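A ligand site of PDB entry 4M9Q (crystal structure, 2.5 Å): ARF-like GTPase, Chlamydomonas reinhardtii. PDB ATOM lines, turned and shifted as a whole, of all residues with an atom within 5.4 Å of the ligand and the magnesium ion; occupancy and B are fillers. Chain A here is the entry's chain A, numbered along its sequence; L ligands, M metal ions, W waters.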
ATOM      1  N   GLY A  11      27.559   1.743 -11.585  1.00  0.00           N
ATOM      2  CA  GLY A  11      27.540   2.578 -10.381  1.00  0.00           C
ATOM      3  C   GLY A  11      26.532   2.029  -9.392  1.00  0.00           C
ATOM      4  O   GLY A  11      25.682   1.264  -9.765  1.00  0.00           O
ATOM      5  N   LEU A  12      26.618   2.455  -8.138  1.00  0.00           N
ATOM      6  CA  LEU A  12      25.799   1.876  -7.080  1.00  0.00           C
ATOM      7  C   LEU A  12      24.340   2.237  -7.310  1.00  0.00           C
ATOM      8  O   LEU A  12      24.011   3.209  -8.023  1.00  0.00           O
ATOM      9  CB  LEU A  12      26.209   2.406  -5.704  1.00  0.00           C
ATOM     10  CG  LEU A  12      27.628   2.166  -5.177  1.00  0.00           C
ATOM     11  CD1 LEU A  12      27.779   2.765  -3.790  1.00  0.00           C
ATOM     12  CD2 LEU A  12      28.019   0.689  -5.203  1.00  0.00           C
ATOM     13  N   ASP A  13      23.460   1.488  -6.667  1.00  0.00           N
ATOM     14  CA  ASP A  13      22.067   1.835  -6.674  1.00  0.00           C
ATOM     15  C   ASP A  13      21.941   3.268  -6.144  1.00  0.00           C
ATOM     16  O   ASP A  13      22.686   3.711  -5.297  1.00  0.00           O
ATOM     17  CB  ASP A  13      21.259   0.864  -5.826  1.00  0.00           C
ATOM     18  CG  ASP A  13      21.675   0.854  -4.395  1.00  0.00           C
ATOM     19  OD1 ASP A  13      22.765   0.301  -4.114  1.00  0.00           O
ATOM     20  OD2 ASP A  13      20.933   1.410  -3.543  1.00  0.00           O
ATOM     21  N   ASN A  14      21.019   4.004  -6.737  1.00  0.00           N
ATOM     22  CA  ASN A  14      20.698   5.361  -6.345  1.00  0.00           C
ATOM     23  C   ASN A  14      21.643   6.446  -6.885  1.00  0.00           C
ATOM     24  O   ASN A  14      21.424   7.637  -6.663  1.00  0.00           O
ATOM     25  CB  ASN A  14      20.545   5.457  -4.816  1.00  0.00           C
ATOM     26  CG  ASN A  14      19.659   6.622  -4.394  1.00  0.00           C
ATOM     27  OD1 ASN A  14      18.522   6.723  -4.860  1.00  0.00           O
ATOM     28  ND2 ASN A  14      20.177   7.516  -3.534  1.00  0.00           N
ATOM     29  N   ALA A  15      22.650   6.034  -7.647  1.00  0.00           N
ATOM     30  CA  ALA A  15      23.659   6.972  -8.119  1.00  0.00           C
ATOM     31  C   ALA A  15      23.060   7.943  -9.158  1.00  0.00           C
ATOM     32  O   ALA A  15      23.455   9.163  -9.229  1.00  0.00           O
ATOM     33  CB  ALA A  15      24.832   6.232  -8.716  1.00  0.00           C
ATOM     34  N   GLY A  16      22.117   7.405  -9.950  1.00  0.00           N
ATOM     35  CA  GLY A  16      21.402   8.175 -10.957  1.00  0.00           C
ATOM     36  C   GLY A  16      21.613   7.756 -12.394  1.00  0.00           C
ATOM     37  O   GLY A  16      21.442   8.588 -13.274  1.00  0.00           O
ATOM     38  N   LYS A  17      21.899   6.465 -12.610  1.00  0.00           N
ATOM     39  CA  LYS A  17      22.261   5.938 -13.920  1.00  0.00           C
ATOM     40  C   LYS A  17      21.054   6.002 -14.848  1.00  0.00           C
ATOM     41  O   LYS A  17      21.127   6.549 -15.950  1.00  0.00           O
ATOM     42  CB  LYS A  17      22.676   4.489 -13.834  1.00  0.00           C
ATOM     43  CG  LYS A  17      23.837   4.245 -12.899  1.00  0.00           C
ATOM     44  CD  LYS A  17      24.222   2.755 -12.818  1.00  0.00           C
ATOM     45  CE  LYS A  17      23.204   1.958 -12.008  1.00  0.00           C
ATOM     46  NZ  LYS A  17      23.245   2.291 -10.560  1.00  0.00           N
ATOM     47  N   THR A  18      19.931   5.456 -14.403  1.00  0.00           N
ATOM     48  CA  THR A  18      18.758   5.438 -15.241  1.00  0.00           C
ATOM     49  C   THR A  18      18.320   6.877 -15.590  1.00  0.00           C
ATOM     50  O   THR A  18      18.031   7.163 -16.737  1.00  0.00           O
ATOM     51  CB  THR A  18      17.663   4.575 -14.626  1.00  0.00           C
ATOM     52  OG1 THR A  18      18.193   3.261 -14.398  1.00  0.00           O
ATOM     53  CG2 THR A  18      16.421   4.412 -15.533  1.00  0.00           C
ATOM     54  N   THR A  19      18.366   7.786 -14.624  1.00  0.00           N
ATOM     55  CA  THR A  19      17.999   9.196 -14.880  1.00  0.00           C
ATOM     56  C   THR A  19      18.995   9.823 -15.849  1.00  0.00           C
ATOM     57  O   THR A  19      18.644  10.589 -16.732  1.00  0.00           O
ATOM     58  CB  THR A  19      17.974   9.976 -13.569  1.00  0.00           C
ATOM     59  OG1 THR A  19      17.167   9.266 -12.600  1.00  0.00           O
ATOM     60  CG2 THR A  19      17.375  11.414 -13.756  1.00  0.00           C
ATOM     61  N   LEU A  20      20.253   9.470 -15.717  1.00  0.00           N
ATOM     62  CA  LEU A  20      21.284  10.007 -16.583  1.00  0.00           C
ATOM     63  C   LEU A  20      21.091   9.496 -18.000  1.00  0.00           C
ATOM     64  O   LEU A  20      21.117  10.244 -18.962  1.00  0.00           O
ATOM     65  CB  LEU A  20      22.641   9.641 -16.034  1.00  0.00           C
ATOM     66  CG  LEU A  20      23.808  10.311 -16.745  1.00  0.00           C
ATOM     67  CD1 LEU A  20      24.898  10.604 -15.708  1.00  0.00           C
ATOM     68  CD2 LEU A  20      24.277   9.403 -17.876  1.00  0.00           C
ATOM     69  N   THR A  32      11.481   7.203 -12.689  1.00  0.00           N
ATOM     70  CA  THR A  32      12.343   6.040 -12.654  1.00  0.00           C
ATOM     71  C   THR A  32      12.130   5.290 -11.367  1.00  0.00           C
ATOM     72  O   THR A  32      11.948   5.893 -10.308  1.00  0.00           O
ATOM     73  CB  THR A  32      13.831   6.428 -12.664  1.00  0.00           C
ATOM     74  OG1 THR A  32      14.119   7.171 -11.479  1.00  0.00           O
ATOM     75  CG2 THR A  32      14.207   7.211 -13.901  1.00  0.00           C
ATOM     76  N   THR A  33      12.203   3.974 -11.456  1.00  0.00           N
ATOM     77  CA  THR A  33      12.196   3.114 -10.274  1.00  0.00           C
ATOM     78  C   THR A  33      13.519   2.392 -10.318  1.00  0.00           C
ATOM     79  O   THR A  33      14.121   2.311 -11.368  1.00  0.00           O
ATOM     80  CB  THR A  33      10.998   2.095 -10.315  1.00  0.00           C
ATOM     81  OG1 THR A  33      10.818   1.581 -11.645  1.00  0.00           O
ATOM     82  CG2 THR A  33       9.661   2.775  -9.896  1.00  0.00           C
ATOM     83  N   PRO A  34      13.957   1.834  -9.202  1.00  0.00           N
ATOM     84  CA  PRO A  34      15.126   0.977  -9.216  1.00  0.00           C
ATOM     85  C   PRO A  34      15.149  -0.050 -10.350  1.00  0.00           C
ATOM     86  O   PRO A  34      14.170  -0.714 -10.634  1.00  0.00           O
ATOM     87  CB  PRO A  34      15.039   0.278  -7.859  1.00  0.00           C
ATOM     88  CG  PRO A  34      14.395   1.306  -6.975  1.00  0.00           C
ATOM     89  CD  PRO A  34      13.348   1.915  -7.860  1.00  0.00           C
ATOM     90  N   THR A  35      16.287  -0.175 -11.007  1.00  0.00           N
ATOM     91  CA  THR A  35      16.422  -1.091 -12.109  1.00  0.00           C
ATOM     92  C   THR A  35      16.759  -2.490 -11.578  1.00  0.00           C
ATOM     93  O   THR A  35      17.829  -2.714 -11.039  1.00  0.00           O
ATOM     94  CB  THR A  35      17.509  -0.553 -13.018  1.00  0.00           C
ATOM     95  OG1 THR A  35      17.186   0.824 -13.311  1.00  0.00           O
ATOM     96  CG2 THR A  35      17.647  -1.379 -14.289  1.00  0.00           C
ATOM     97  N   ASN A  39      18.093  -1.521 -18.728  1.00  0.00           N
ATOM     98  CA  ASN A  39      17.565  -0.719 -19.817  1.00  0.00           C
ATOM     99  C   ASN A  39      18.693  -0.630 -20.865  1.00  0.00           C
ATOM    100  O   ASN A  39      19.866  -0.664 -20.526  1.00  0.00           O
ATOM    101  CB  ASN A  39      17.221   0.667 -19.268  1.00  0.00           C
ATOM    102  CG  ASN A  39      16.275   0.611 -18.041  1.00  0.00           C
ATOM    103  OD1 ASN A  39      15.187   0.040 -18.106  1.00  0.00           O
ATOM    104  ND2 ASN A  39      16.690   1.222 -16.937  1.00  0.00           N
ATOM    105  N   ASP A  54      22.206   0.135 -19.308  1.00  0.00           N
ATOM    106  CA  ASP A  54      22.015   0.676 -17.983  1.00  0.00           C
ATOM    107  C   ASP A  54      21.686  -0.483 -17.039  1.00  0.00           C
ATOM    108  O   ASP A  54      20.606  -1.014 -17.082  1.00  0.00           O
ATOM    109  CB  ASP A  54      20.906   1.719 -18.038  1.00  0.00           C
ATOM    110  CG  ASP A  54      20.337   2.066 -16.663  1.00  0.00           C
ATOM    111  OD1 ASP A  54      21.068   1.999 -15.646  1.00  0.00           O
ATOM    112  OD2 ASP A  54      19.140   2.428 -16.600  1.00  0.00           O
ATOM    113  N   LEU A  55      22.638  -0.904 -16.239  1.00  0.00           N
ATOM    114  CA  LEU A  55      22.482  -2.058 -15.382  1.00  0.00           C
ATOM    115  C   LEU A  55      22.070  -1.606 -13.998  1.00  0.00           C
ATOM    116  O   LEU A  55      22.527  -0.582 -13.516  1.00  0.00           O
ATOM    117  CB  LEU A  55      23.796  -2.801 -15.276  1.00  0.00           C
ATOM    118  CG  LEU A  55      24.143  -3.760 -16.405  1.00  0.00           C
ATOM    119  CD1 LEU A  55      23.327  -3.515 -17.691  1.00  0.00           C
ATOM    120  CD2 LEU A  55      25.631  -3.774 -16.687  1.00  0.00           C
ATOM    121  N   GLY A  56      21.251  -2.396 -13.324  1.00  0.00           N
ATOM    122  CA  GLY A  56      20.900  -2.092 -11.944  1.00  0.00           C
ATOM    123  C   GLY A  56      22.113  -2.123 -11.055  1.00  0.00           C
ATOM    124  O   GLY A  56      23.026  -2.910 -11.308  1.00  0.00           O
ATOM    125  N   GLY A  57      22.138  -1.276 -10.024  1.00  0.00           N
ATOM    126  CA  GLY A  57      23.233  -1.229  -9.102  1.00  0.00           C
ATOM    127  C   GLY A  57      23.003  -1.795  -7.718  1.00  0.00           C
ATOM    128  O   GLY A  57      23.928  -1.806  -6.924  1.00  0.00           O
ATOM    129  N   GLY A  58      21.811  -2.275  -7.395  1.00  0.00           N
ATOM    130  CA  GLY A  58      21.553  -2.897  -6.107  1.00  0.00           C
ATOM    131  C   GLY A  58      22.502  -4.042  -5.832  1.00  0.00           C
ATOM    132  O   GLY A  58      22.937  -4.706  -6.761  1.00  0.00           O
ATOM    133  N   ASN A 113      27.609  12.752  -9.933  1.00  0.00           N
ATOM    134  CA  ASN A 113      26.231  13.186 -10.127  1.00  0.00           C
ATOM    135  C   ASN A 113      25.589  13.896  -8.910  1.00  0.00           C
ATOM    136  O   ASN A 113      26.093  13.867  -7.794  1.00  0.00           O
ATOM    137  CB  ASN A 113      25.390  11.981 -10.542  1.00  0.00           C
ATOM    138  CG  ASN A 113      24.022  12.371 -11.037  1.00  0.00           C
ATOM    139  OD1 ASN A 113      23.851  13.401 -11.718  1.00  0.00           O
ATOM    140  ND2 ASN A 113      23.029  11.570 -10.692  1.00  0.00           N
ATOM    141  N   LYS A 114      24.492  14.583  -9.165  1.00  0.00           N
ATOM    142  CA  LYS A 114      23.676  15.219  -8.094  1.00  0.00           C
ATOM    143  C   LYS A 114      24.326  16.510  -7.555  1.00  0.00           C
ATOM    144  O   LYS A 114      24.266  16.771  -6.377  1.00  0.00           O
ATOM    145  CB  LYS A 114      23.390  14.219  -6.974  1.00  0.00           C
ATOM    146  CG  LYS A 114      22.769  12.877  -7.453  1.00  0.00           C
ATOM    147  CD  LYS A 114      21.880  12.242  -6.381  1.00  0.00           C
ATOM    148  CE  LYS A 114      21.440  10.836  -6.720  1.00  0.00           C
ATOM    149  NZ  LYS A 114      20.812  10.100  -5.589  1.00  0.00           N
ATOM    150  N   GLN A 115      24.916  17.299  -8.444  1.00  0.00           N
ATOM    151  CA  GLN A 115      25.566  18.538  -8.080  1.00  0.00           C
ATOM    152  C   GLN A 115      24.604  19.658  -7.712  1.00  0.00           C
ATOM    153  O   GLN A 115      25.038  20.711  -7.294  1.00  0.00           O
ATOM    154  CB  GLN A 115      26.486  19.025  -9.171  1.00  0.00           C
ATOM    155  CG  GLN A 115      27.677  18.117  -9.482  1.00  0.00           C
ATOM    156  CD  GLN A 115      28.755  18.143  -8.432  1.00  0.00           C
ATOM    157  OE1 GLN A 115      29.047  19.184  -7.908  1.00  0.00           O
ATOM    158  NE2 GLN A 115      29.356  17.011  -8.155  1.00  0.00           N
ATOM    159  N   ASP A 116      23.301  19.419  -7.888  1.00  0.00           N
ATOM    160  CA  ASP A 116      22.266  20.332  -7.363  1.00  0.00           C
ATOM    161  C   ASP A 116      22.081  20.175  -5.869  1.00  0.00           C
ATOM    162  O   ASP A 116      21.539  21.056  -5.202  1.00  0.00           O
ATOM    163  CB  ASP A 116      20.910  20.083  -8.037  1.00  0.00           C
ATOM    164  CG  ASP A 116      20.444  18.629  -7.866  1.00  0.00           C
ATOM    165  OD1 ASP A 116      21.224  17.635  -8.097  1.00  0.00           O
ATOM    166  OD2 ASP A 116      19.256  18.458  -7.475  1.00  0.00           O
ATOM    167  N   LEU A 117      22.488  19.047  -5.312  1.00  0.00           N
ATOM    168  CA  LEU A 117      22.341  18.871  -3.838  1.00  0.00           C
ATOM    169  C   LEU A 117      23.419  19.644  -3.052  1.00  0.00           C
ATOM    170  O   LEU A 117      24.602  19.664  -3.405  1.00  0.00           O
ATOM    171  CB  LEU A 117      22.343  17.384  -3.476  1.00  0.00           C
ATOM    172  CG  LEU A 117      21.088  16.670  -3.992  1.00  0.00           C
ATOM    173  CD1 LEU A 117      21.217  15.203  -3.593  1.00  0.00           C
ATOM    174  CD2 LEU A 117      19.816  17.377  -3.464  1.00  0.00           C
ATOM    175  N   CYS A 144      27.990  16.588 -12.645  1.00  0.00           N
ATOM    176  CA  CYS A 144      26.791  16.767 -13.445  1.00  0.00           C
ATOM    177  C   CYS A 144      25.552  16.699 -12.597  1.00  0.00           C
ATOM    178  O   CYS A 144      25.595  16.416 -11.388  1.00  0.00           O
ATOM    179  CB  CYS A 144      26.707  15.689 -14.520  1.00  0.00           C
ATOM    180  SG  CYS A 144      26.470  14.072 -13.787  1.00  0.00           S
ATOM    181  N   THR A 145      24.432  16.960 -13.258  1.00  0.00           N
ATOM    182  CA  THR A 145      23.096  16.914 -12.653  1.00  0.00           C
ATOM    183  C   THR A 145      22.172  16.258 -13.641  1.00  0.00           C
ATOM    184  O   THR A 145      21.671  16.867 -14.571  1.00  0.00           O
ATOM    185  CB  THR A 145      22.653  18.361 -12.325  1.00  0.00           C
ATOM    186  OG1 THR A 145      23.650  18.915 -11.486  1.00  0.00           O
ATOM    187  CG2 THR A 145      21.304  18.410 -11.641  1.00  0.00           C
ATOM    188  N   ALA A 146      22.016  14.971 -13.483  1.00  0.00           N
ATOM    189  CA  ALA A 146      21.231  14.153 -14.375  1.00  0.00           C
ATOM    190  C   ALA A 146      19.773  14.575 -14.255  1.00  0.00           C
ATOM    191  O   ALA A 146      19.020  14.384 -15.188  1.00  0.00           O
ATOM    192  CB  ALA A 146      21.383  12.679 -13.981  1.00  0.00           C
ATOM    193  N   LYS A 147      19.363  15.113 -13.123  1.00  0.00           N
ATOM    194  CA  LYS A 147      17.985  15.564 -12.934  1.00  0.00           C
ATOM    195  C   LYS A 147      17.935  17.077 -12.777  1.00  0.00           C
ATOM    196  O   LYS A 147      17.835  17.588 -11.660  1.00  0.00           O
ATOM    197  CB  LYS A 147      17.358  14.896 -11.685  1.00  0.00           C
ATOM    198  CG  LYS A 147      15.836  14.998 -11.618  1.00  0.00           C
ATOM    199  CD  LYS A 147      15.276  14.518 -10.291  1.00  0.00           C
ATOM    200  CE  LYS A 147      13.771  14.799 -10.143  1.00  0.00           C
ATOM    201  NZ  LYS A 147      13.420  15.582  -8.917  1.00  0.00           N
HETATM  202  P1  LIG L   1      19.460   1.579  -9.666  1.00  0.00           P
HETATM  203  O1  LIG L   1      18.502   1.431 -10.969  1.00  0.00           O
HETATM  204  O2  LIG L   1      20.959   1.279 -10.020  1.00  0.00           O
HETATM  205  O3  LIG L   1      18.830   0.706  -8.563  1.00  0.00           O
HETATM  206  N1  LIG L   1      19.476   3.224  -9.261  1.00  0.00           N
HETATM  207  P2  LIG L   1      19.855   4.335 -10.477  1.00  0.00           P
HETATM  208  O4  LIG L   1      19.314   3.891 -11.927  1.00  0.00           O
HETATM  209  O5  LIG L   1      21.354   4.508 -10.430  1.00  0.00           O
HETATM  210  O6  LIG L   1      19.154   5.650  -9.917  1.00  0.00           O
HETATM  211  P3  LIG L   1      18.010   6.509 -10.600  1.00  0.00           P
HETATM  212  O7  LIG L   1      16.847   5.611 -10.479  1.00  0.00           O
HETATM  213  O8  LIG L   1      18.527   6.992 -11.915  1.00  0.00           O
HETATM  214  O9  LIG L   1      17.970   7.709  -9.556  1.00  0.00           O
HETATM  215  C1  LIG L   1      17.881   7.414  -8.135  1.00  0.00           C
HETATM  216  C2  LIG L   1      17.182   8.581  -7.391  1.00  0.00           C
HETATM  217  O10 LIG L   1      18.019   9.735  -7.538  1.00  0.00           O
HETATM  218  C3  LIG L   1      15.873   9.031  -8.017  1.00  0.00           C
HETATM  219  O11 LIG L   1      15.031   9.742  -7.105  1.00  0.00           O
HETATM  220  C4  LIG L   1      16.286  10.083  -8.993  1.00  0.00           C
HETATM  221  O12 LIG L   1      15.295  11.015  -9.303  1.00  0.00           O
HETATM  222  C5  LIG L   1      17.340  10.789  -8.194  1.00  0.00           C
HETATM  223  N2  LIG L   1      18.301  11.586  -8.961  1.00  0.00           N
HETATM  224  C6  LIG L   1      18.956  11.166 -10.041  1.00  0.00           C
HETATM  225  N3  LIG L   1      19.805  12.108 -10.477  1.00  0.00           N
HETATM  226  C7  LIG L   1      19.681  13.164  -9.671  1.00  0.00           C
HETATM  227  C8  LIG L   1      20.294  14.502  -9.632  1.00  0.00           C
HETATM  228  O13 LIG L   1      21.141  14.863 -10.473  1.00  0.00           O
HETATM  229  N4  LIG L   1      19.942  15.298  -8.650  1.00  0.00           N
HETATM  230  C9  LIG L   1      19.021  14.941  -7.697  1.00  0.00           C
HETATM  231  N5  LIG L   1      18.726  15.853  -6.767  1.00  0.00           N
HETATM  232  N6  LIG L   1      18.398  13.729  -7.666  1.00  0.00           N
HETATM  233  C10 LIG L   1      18.676  12.825  -8.663  1.00  0.00           C
HETATM  234 MG    MG M   1      18.325   2.373 -12.736  1.00  0.00          MG
HETATM  235  O   HOH W   1      20.029   1.444 -13.354  1.00  0.00           O
HETATM  236  O   HOH W   2      16.596   3.339 -12.080  1.00  0.00           O
HETATM  237  O   HOH W   3      18.731  11.729  -4.974  1.00  0.00           O
HETATM  238  O   HOH W   4      14.534  10.235 -11.958  1.00  0.00           O
HETATM  239  O   HOH W   5      19.215  -1.917  -8.765  1.00  0.00           O
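OD2 of Asp 54 touches the magnesium ion, 3.9 Å away. Three residues have an atom within 4 Å of the magnesium ion: Thr 18, Thr 35 and Asp 54. Along chain A the residues within 4 Å of the magnesium ion span positions 18 to 54. The nearest printed residue that does not touch the magnesium ion is Thr 33 (4.4 Å).
The magnesium ion is bound by OG1 of Thr 18 (1.9 Å), O4 of the ligand (2.0 Å), OG1 of Thr 35 (2.0 Å), O1 of the ligand (2.0 Å), water W1 (2.0 Å) and water W2 (2.1 Å). The magnesium ion has six donor atoms within binding distance.
Water W2 bridges O of Thr 33 and O7 of the ligand. Water W1 lies within hydrogen-bond range of the side-chain carboxylate (OD1) of Asp 54 (2.6 Å), the backbone carbonyl oxygen (O) of Leu 55 (3.2 Å) and an oxygen (O2) of the ligand (3.5 Å). Water W5 lies within hydrogen-bond range of an oxygen (O3) of the ligand (2.7 Å), the backbone carbonyl oxygen of Thr 35 (2.8 Å), the backbone NH of Gly 58 (3.0 Å) and the backbone NH of Gly 57 (3.2 Å). Water W4 lies within hydrogen-bond range of O12 of the ligand (2.9 Å), OG1 of Thr 19 (2.9 Å) and OG1 of Thr 32 (3.1 Å). Water W3 bridges the side-chain amino group of Lys 114 (2.7 Å) and an oxygen (O10) of the ligand (3.3 Å).
The side-chain hydroxyl of Thr 18 sits close to the side-chain carboxylate of Asp 54, 2.5 Å away. The side-chain amino group of Lys 17 lies within hydrogen-bond range of the backbone carbonyl oxygen of Leu 12 (2.8 Å). The backbone carbonyl oxygen of Gly 11 is in hydrogen-bond range of the side-chain amino group of Lys 17 (2.8 Å). The backbone carbonyl oxygen (O) of Gly 57 is in hydrogen-bond range of the backbone NH (N) of Asp 13 (3.3 Å). NZ of Lys 114 sits at hydrogen-bond distance from O of Asn 14, 2.8 Å away. The side-chain amide nitrogen of Asn 113 lies within hydrogen-bond range of the backbone carbonyl oxygen of Ala 15. N of Lys 114 is in hydrogen-bond range of O of Cys 144 (3.1 Å). The side-chain carboxylate (OD2) of Asp 54 sits at hydrogen-bond distance from the side-chain amide nitrogen (ND2) of Asn 39, at 2.8 Å.
The backbone NH of Thr 18 is in hydrogen-bond range of an oxygen (O8) of the ligand, 3.2 Å away. The backbone NH (N) of Thr 35 lies close to an oxygen (O1) of the ligand, at 2.7 Å. N of Lys 17 is in hydrogen-bond range of O5 of the ligand (3.0 Å). The side-chain amino group of Lys 17 lies within salt-bridge range of an oxygen (O2) of the ligand. The side-chain carboxylate (OD1) of Asp 116 is in hydrogen-bond range of a nitrogen (N4) of the ligand (2.7 Å). N of Thr 19 sits at hydrogen-bond distance from O8 of the ligand (2.8 Å). OG1 of Thr 19 is in hydrogen-bond range of O8 of the ligand (2.7 Å). An oxygen (O2) of the ligand lies within hydrogen-bond range of the backbone NH (N) of Gly 57 (2.8 Å). O5 of the ligand lies within hydrogen-bond range of N of Gly 16. The backbone NH (N) of Ala 146 is in hydrogen-bond range of an oxygen (O13) of the ligand, 3.1 Å away. O13 of the ligand is in hydrogen-bond range of N of Lys 147 (3.2 Å). A nitrogen (N3) of the ligand lies within hydrogen-bond range of the side-chain amide nitrogen (ND2) of Asn 113, at 3.3 Å. The side-chain hydroxyl of Thr 32 is in hydrogen-bond range of an oxygen (O7) of the ligand (3.3 Å). The side-chain amino group of Lys 114 is in hydrogen-bond range of an oxygen (O10) of the ligand (3.4 Å). An oxygen (O5) of the ligand sits at hydrogen-bond distance from the backbone NH (N) of Ala 15, at 3.4 Å.
N1 of the ligand sits close to N of Asn 14 (3.1 Å). Leu 12 touches the ligand (O to O5, 3.8 Å). Asp 13 touches the ligand (CA to O2, 3.6 Å). Pro 34 touches the ligand (C to O1, 3.7 Å). Gly 56 touches the ligand. CG of Leu 117 touches N5 of the ligand, 3.7 Å away. Thr 145 touches the ligand. Hydrophobic or aromatic side chains within 4 Å of the ligand: Pro 34, Leu 117 and Ala 146. Along chain A the residues within 4 Å of the ligand span positions 12 to 147.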
